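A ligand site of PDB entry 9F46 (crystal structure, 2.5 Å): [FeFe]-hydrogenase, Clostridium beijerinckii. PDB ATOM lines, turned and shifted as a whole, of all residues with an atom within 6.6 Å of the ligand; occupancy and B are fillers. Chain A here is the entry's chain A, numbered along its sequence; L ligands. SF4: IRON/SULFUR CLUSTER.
The side-chain sulfur (SG) of Cys 368 binds an iron atom (FE3) of the ligand, 2.3 Å away. An iron atom (FE1) of the ligand is bound by the side-chain sulfur of Cys 423 (2.2 Å). The side-chain sulfur (SG) of Cys 567 binds an iron atom (FE2) of the ligand. The side-chain sulfur of Cys 571 binds an iron atom (FE4) of the ligand (2.3 Å).
Pro 422 touches the ligand. Ala 566 touches the ligand (N to S1, 3.9 Å). Gly 574 touches the ligand (CA to S3, 3.8 Å). Hydrophobic or aromatic side chains that line the ligand: Pro 422. The nearest printed residue that does not touch the ligand is Met 565 (4.02 Å).
The side-chain sulfur (SG) of Cys 423 sits close to the backbone NH (N) of Ala 425, at 3.7 Å. The backbone NH of Ser 370 sits close to the side-chain sulfur of Cys 368. The backbone NH (N) of Cys 368 lies within hydrogen-bond range of the side-chain hydroxyl (OG) of Ser 366, 3.2 Å away. N of Lys 426 sits close to SG of Cys 423 (3.4 Å). The backbone carbonyl oxygen (O) of Gly 486 sits at hydrogen-bond distance from the backbone NH (N) of Cys 571, at 3.0 Å. The backbone carbonyl oxygen (O) of Pro 422 lies within hydrogen-bond range of the backbone NH (N) of Gly 575 (3.4 Å). N of Ala 566 sits close to SG of Cys 368, at 3.7 Å.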
ATOM      1  N   HIS A 254      33.788  20.931 -23.037  1.00  0.00           N
ATOM      2  CA  HIS A 254      33.142  20.025 -23.985  1.00  0.00           C
ATOM      3  C   HIS A 254      31.732  20.507 -24.354  1.00  0.00           C
ATOM      4  O   HIS A 254      30.877  19.709 -24.730  1.00  0.00           O
ATOM      5  CB  HIS A 254      33.091  18.598 -23.445  1.00  0.00           C
ATOM      6  CG  HIS A 254      34.431  17.948 -23.315  1.00  0.00           C
ATOM      7  ND1 HIS A 254      35.233  18.115 -22.211  1.00  0.00           N
ATOM      8  CD2 HIS A 254      35.120  17.155 -24.166  1.00  0.00           C
ATOM      9  CE1 HIS A 254      36.355  17.432 -22.371  1.00  0.00           C
ATOM     10  NE2 HIS A 254      36.315  16.844 -23.556  1.00  0.00           N
ATOM     11  N   CYS A 255      31.511  21.821 -24.261  1.00  0.00           N
ATOM     12  CA  CYS A 255      30.222  22.377 -24.645  1.00  0.00           C
ATOM     13  C   CYS A 255      29.930  22.181 -26.124  1.00  0.00           C
ATOM     14  O   CYS A 255      28.762  22.230 -26.528  1.00  0.00           O
ATOM     15  CB  CYS A 255      30.173  23.877 -24.299  1.00  0.00           C
ATOM     16  SG  CYS A 255      31.061  24.938 -25.463  1.00  0.00           S
ATOM     17  N   GLY A 256      30.959  21.969 -26.937  1.00  0.00           N
ATOM     18  CA  GLY A 256      30.785  21.669 -28.333  1.00  0.00           C
ATOM     19  C   GLY A 256      30.478  22.847 -29.218  1.00  0.00           C
ATOM     20  O   GLY A 256      30.116  22.645 -30.384  1.00  0.00           O
ATOM     21  N   SER A 366      21.443  20.145 -12.578  1.00  0.00           N
ATOM     22  CA  SER A 366      21.573  20.153 -14.026  1.00  0.00           C
ATOM     23  C   SER A 366      22.319  18.910 -14.474  1.00  0.00           C
ATOM     24  O   SER A 366      23.335  18.544 -13.875  1.00  0.00           O
ATOM     25  CB  SER A 366      22.299  21.412 -14.510  1.00  0.00           C
ATOM     26  OG  SER A 366      22.676  21.294 -15.871  1.00  0.00           O
ATOM     27  N   CYS A 367      21.825  18.279 -15.537  1.00  0.00           N
ATOM     28  CA  CYS A 367      22.449  17.098 -16.098  1.00  0.00           C
ATOM     29  C   CYS A 367      23.579  17.421 -17.071  1.00  0.00           C
ATOM     30  O   CYS A 367      24.177  16.503 -17.628  1.00  0.00           O
ATOM     31  CB  CYS A 367      21.390  16.251 -16.816  1.00  0.00           C
ATOM     32  SG  CYS A 367      20.417  17.200 -18.002  1.00  0.00           S
ATOM     33  N   CYS A 368      23.873  18.704 -17.274  1.00  0.00           N
ATOM     34  CA  CYS A 368      24.861  19.108 -18.259  1.00  0.00           C
ATOM     35  C   CYS A 368      26.275  18.922 -17.718  1.00  0.00           C
ATOM     36  O   CYS A 368      26.603  19.504 -16.677  1.00  0.00           O
ATOM     37  CB  CYS A 368      24.644  20.565 -18.646  1.00  0.00           C
ATOM     38  SG  CYS A 368      25.780  21.190 -19.896  1.00  0.00           S
ATOM     39  N   PRO A 369      27.139  18.144 -18.377  1.00  0.00           N
ATOM     40  CA  PRO A 369      28.510  17.994 -17.874  1.00  0.00           C
ATOM     41  C   PRO A 369      29.311  19.283 -17.921  1.00  0.00           C
ATOM     42  O   PRO A 369      30.244  19.445 -17.123  1.00  0.00           O
ATOM     43  CB  PRO A 369      29.134  16.927 -18.784  1.00  0.00           C
ATOM     44  CG  PRO A 369      27.974  16.315 -19.545  1.00  0.00           C
ATOM     45  CD  PRO A 369      26.899  17.350 -19.594  1.00  0.00           C
ATOM     46  N   SER A 370      28.960  20.211 -18.817  1.00  0.00           N
ATOM     47  CA  SER A 370      29.835  21.347 -19.089  1.00  0.00           C
ATOM     48  C   SER A 370      30.057  22.210 -17.860  1.00  0.00           C
ATOM     49  O   SER A 370      31.084  22.905 -17.773  1.00  0.00           O
ATOM     50  CB  SER A 370      29.259  22.181 -20.225  1.00  0.00           C
ATOM     51  OG  SER A 370      29.316  21.486 -21.455  1.00  0.00           O
ATOM     52  N   PRO A 422      22.269  14.293 -27.418  1.00  0.00           N
ATOM     53  CA  PRO A 422      22.350  15.379 -28.393  1.00  0.00           C
ATOM     54  C   PRO A 422      23.680  16.116 -28.451  1.00  0.00           C
ATOM     55  O   PRO A 422      23.739  17.180 -29.085  1.00  0.00           O
ATOM     56  CB  PRO A 422      21.237  16.325 -27.941  1.00  0.00           C
ATOM     57  CG  PRO A 422      21.179  16.145 -26.428  1.00  0.00           C
ATOM     58  CD  PRO A 422      21.706  14.739 -26.125  1.00  0.00           C
ATOM     59  N   CYS A 423      24.742  15.629 -27.815  1.00  0.00           N
ATOM     60  CA  CYS A 423      25.924  16.451 -27.625  1.00  0.00           C
ATOM     61  C   CYS A 423      27.165  15.602 -27.452  1.00  0.00           C
ATOM     62  O   CYS A 423      27.101  14.411 -27.119  1.00  0.00           O
ATOM     63  CB  CYS A 423      25.756  17.385 -26.417  1.00  0.00           C
ATOM     64  SG  CYS A 423      25.624  16.490 -24.857  1.00  0.00           S
ATOM     65  N   ILE A 424      28.317  16.241 -27.662  1.00  0.00           N
ATOM     66  CA  ILE A 424      29.601  15.591 -27.369  1.00  0.00           C
ATOM     67  C   ILE A 424      29.913  15.569 -25.882  1.00  0.00           C
ATOM     68  O   ILE A 424      30.706  14.729 -25.427  1.00  0.00           O
ATOM     69  CB  ILE A 424      30.755  16.288 -28.129  1.00  0.00           C
ATOM     70  CG1 ILE A 424      31.047  17.662 -27.520  1.00  0.00           C
ATOM     71  CG2 ILE A 424      30.416  16.415 -29.603  1.00  0.00           C
ATOM     72  CD1 ILE A 424      31.937  18.566 -28.396  1.00  0.00           C
ATOM     73  N   ALA A 425      29.325  16.485 -25.105  1.00  0.00           N
ATOM     74  CA  ALA A 425      29.591  16.489 -23.666  1.00  0.00           C
ATOM     75  C   ALA A 425      29.164  15.182 -23.016  1.00  0.00           C
ATOM     76  O   ALA A 425      29.798  14.728 -22.060  1.00  0.00           O
ATOM     77  CB  ALA A 425      28.877  17.670 -23.010  1.00  0.00           C
ATOM     78  N   LYS A 426      28.113  14.545 -23.542  1.00  0.00           N
ATOM     79  CA  LYS A 426      27.725  13.244 -23.015  1.00  0.00           C
ATOM     80  C   LYS A 426      28.708  12.163 -23.422  1.00  0.00           C
ATOM     81  O   LYS A 426      28.926  11.206 -22.670  1.00  0.00           O
ATOM     82  CB  LYS A 426      26.310  12.892 -23.460  1.00  0.00           C
ATOM     83  CG  LYS A 426      25.239  13.741 -22.780  1.00  0.00           C
ATOM     84  CD  LYS A 426      25.164  13.450 -21.277  1.00  0.00           C
ATOM     85  CE  LYS A 426      24.170  14.368 -20.581  1.00  0.00           C
ATOM     86  NZ  LYS A 426      24.298  14.335 -19.105  1.00  0.00           N
ATOM     87  N   PHE A 485      13.367  17.841 -18.758  1.00  0.00           N
ATOM     88  CA  PHE A 485      14.823  17.955 -18.597  1.00  0.00           C
ATOM     89  C   PHE A 485      15.491  18.456 -19.866  1.00  0.00           C
ATOM     90  O   PHE A 485      16.563  19.071 -19.812  1.00  0.00           O
ATOM     91  CB  PHE A 485      15.423  16.599 -18.227  1.00  0.00           C
ATOM     92  CG  PHE A 485      15.578  16.366 -16.755  1.00  0.00           C
ATOM     93  CD1 PHE A 485      14.493  16.471 -15.901  1.00  0.00           C
ATOM     94  CD2 PHE A 485      16.813  16.031 -16.217  1.00  0.00           C
ATOM     95  CE1 PHE A 485      14.638  16.262 -14.548  1.00  0.00           C
ATOM     96  CE2 PHE A 485      16.965  15.809 -14.864  1.00  0.00           C
ATOM     97  CZ  PHE A 485      15.873  15.926 -14.030  1.00  0.00           C
ATOM     98  N   GLY A 486      14.885  18.190 -21.031  1.00  0.00           N
ATOM     99  CA  GLY A 486      15.526  18.425 -22.301  1.00  0.00           C
ATOM    100  C   GLY A 486      15.573  19.865 -22.771  1.00  0.00           C
ATOM    101  O   GLY A 486      16.184  20.133 -23.809  1.00  0.00           O
ATOM    102  N   ILE A 564      22.054  25.376 -14.713  1.00  0.00           N
ATOM    103  CA  ILE A 564      22.977  25.844 -15.745  1.00  0.00           C
ATOM    104  C   ILE A 564      22.947  24.851 -16.904  1.00  0.00           C
ATOM    105  O   ILE A 564      23.151  23.662 -16.704  1.00  0.00           O
ATOM    106  CB  ILE A 564      24.407  26.012 -15.211  1.00  0.00           C
ATOM    107  CG1 ILE A 564      24.463  27.163 -14.193  1.00  0.00           C
ATOM    108  CG2 ILE A 564      25.370  26.275 -16.357  1.00  0.00           C
ATOM    109  CD1 ILE A 564      25.835  27.468 -13.655  1.00  0.00           C
ATOM    110  N   MET A 565      22.678  25.358 -18.108  1.00  0.00           N
ATOM    111  CA  MET A 565      22.754  24.592 -19.340  1.00  0.00           C
ATOM    112  C   MET A 565      23.734  25.274 -20.282  1.00  0.00           C
ATOM    113  O   MET A 565      23.760  26.502 -20.382  1.00  0.00           O
ATOM    114  CB  MET A 565      21.384  24.466 -20.016  1.00  0.00           C
ATOM    115  CG  MET A 565      20.399  23.584 -19.265  1.00  0.00           C
ATOM    116  SD  MET A 565      20.845  21.834 -19.272  1.00  0.00           S
ATOM    117  CE  MET A 565      19.774  21.207 -17.995  1.00  0.00           C
ATOM    118  N   ALA A 566      24.559  24.478 -20.959  1.00  0.00           N
ATOM    119  CA  ALA A 566      25.579  25.051 -21.844  1.00  0.00           C
ATOM    120  C   ALA A 566      24.990  25.508 -23.173  1.00  0.00           C
ATOM    121  O   ALA A 566      25.484  26.476 -23.759  1.00  0.00           O
ATOM    122  CB  ALA A 566      26.692  24.043 -22.077  1.00  0.00           C
ATOM    123  N   CYS A 567      23.950  24.836 -23.670  1.00  0.00           N
ATOM    124  CA  CYS A 567      23.393  25.134 -24.972  1.00  0.00           C
ATOM    125  C   CYS A 567      22.192  26.055 -24.836  1.00  0.00           C
ATOM    126  O   CYS A 567      21.411  25.950 -23.878  1.00  0.00           O
ATOM    127  CB  CYS A 567      22.979  23.854 -25.685  1.00  0.00           C
ATOM    128  SG  CYS A 567      24.341  22.727 -26.061  1.00  0.00           S
ATOM    129  N   VAL A 568      22.046  26.975 -25.802  1.00  0.00           N
ATOM    130  CA  VAL A 568      20.881  27.841 -25.838  1.00  0.00           C
ATOM    131  C   VAL A 568      19.636  26.988 -26.026  1.00  0.00           C
ATOM    132  O   VAL A 568      19.539  26.200 -26.970  1.00  0.00           O
ATOM    133  CB  VAL A 568      21.024  28.883 -26.947  1.00  0.00           C
ATOM    134  CG1 VAL A 568      19.794  29.781 -27.020  1.00  0.00           C
ATOM    135  CG2 VAL A 568      22.284  29.710 -26.720  1.00  0.00           C
ATOM    136  N   GLY A 570      18.721  24.717 -23.890  1.00  0.00           N
ATOM    137  CA  GLY A 570      18.932  23.423 -23.271  1.00  0.00           C
ATOM    138  C   GLY A 570      19.291  22.340 -24.269  1.00  0.00           C
ATOM    139  O   GLY A 570      19.802  22.601 -25.363  1.00  0.00           O
ATOM    140  N   CYS A 571      19.001  21.100 -23.876  1.00  0.00           N
ATOM    141  CA  CYS A 571      19.480  19.957 -24.640  1.00  0.00           C
ATOM    142  C   CYS A 571      18.855  19.886 -26.032  1.00  0.00           C
ATOM    143  O   CYS A 571      19.464  19.331 -26.948  1.00  0.00           O
ATOM    144  CB  CYS A 571      19.201  18.663 -23.867  1.00  0.00           C
ATOM    145  SG  CYS A 571      20.107  18.574 -22.320  1.00  0.00           S
ATOM    146  N   ILE A 572      17.648  20.437 -26.209  1.00  0.00           N
ATOM    147  CA  ILE A 572      17.064  20.448 -27.553  1.00  0.00           C
ATOM    148  C   ILE A 572      17.952  21.235 -28.520  1.00  0.00           C
ATOM    149  O   ILE A 572      17.816  21.082 -29.736  1.00  0.00           O
ATOM    150  CB  ILE A 572      15.629  21.015 -27.549  1.00  0.00           C
ATOM    151  CG1 ILE A 572      15.539  22.289 -26.712  1.00  0.00           C
ATOM    152  CG2 ILE A 572      14.646  19.961 -27.040  1.00  0.00           C
ATOM    153  CD1 ILE A 572      15.903  23.554 -27.479  1.00  0.00           C
ATOM    154  N   GLY A 573      18.850  22.072 -27.995  1.00  0.00           N
ATOM    155  CA  GLY A 573      19.757  22.833 -28.833  1.00  0.00           C
ATOM    156  C   GLY A 573      21.178  22.291 -28.856  1.00  0.00           C
ATOM    157  O   GLY A 573      22.122  23.022 -29.185  1.00  0.00           O
ATOM    158  N   GLY A 574      21.342  21.022 -28.505  1.00  0.00           N
ATOM    159  CA  GLY A 574      22.673  20.449 -28.444  1.00  0.00           C
ATOM    160  C   GLY A 574      23.321  20.353 -29.817  1.00  0.00           C
ATOM    161  O   GLY A 574      22.656  20.267 -30.847  1.00  0.00           O
ATOM    162  N   GLY A 575      24.657  20.359 -29.811  1.00  0.00           N
ATOM    163  CA  GLY A 575      25.418  20.321 -31.040  1.00  0.00           C
ATOM    164  C   GLY A 575      25.296  19.035 -31.816  1.00  0.00           C
ATOM    165  O   GLY A 575      25.557  19.021 -33.021  1.00  0.00           O
HETATM  166 FE1  SF4 L   1      24.752  18.309 -23.917  1.00  0.00          FE
HETATM  167 FE2  SF4 L   1      23.964  21.124 -24.515  1.00  0.00          FE
HETATM  168 FE3  SF4 L   1      24.728  20.343 -21.715  1.00  0.00          FE
HETATM  169 FE4  SF4 L   1      22.156  19.325 -22.922  1.00  0.00          FE
HETATM  170  S1  SF4 L   1      23.015  21.253 -22.606  1.00  0.00           S
HETATM  171  S2  SF4 L   1      23.852  18.422 -21.991  1.00  0.00           S
HETATM  172  S3  SF4 L   1      23.069  19.219 -24.849  1.00  0.00           S
HETATM  173  S4  SF4 L   1      25.676  20.214 -23.624  1.00  0.00           S
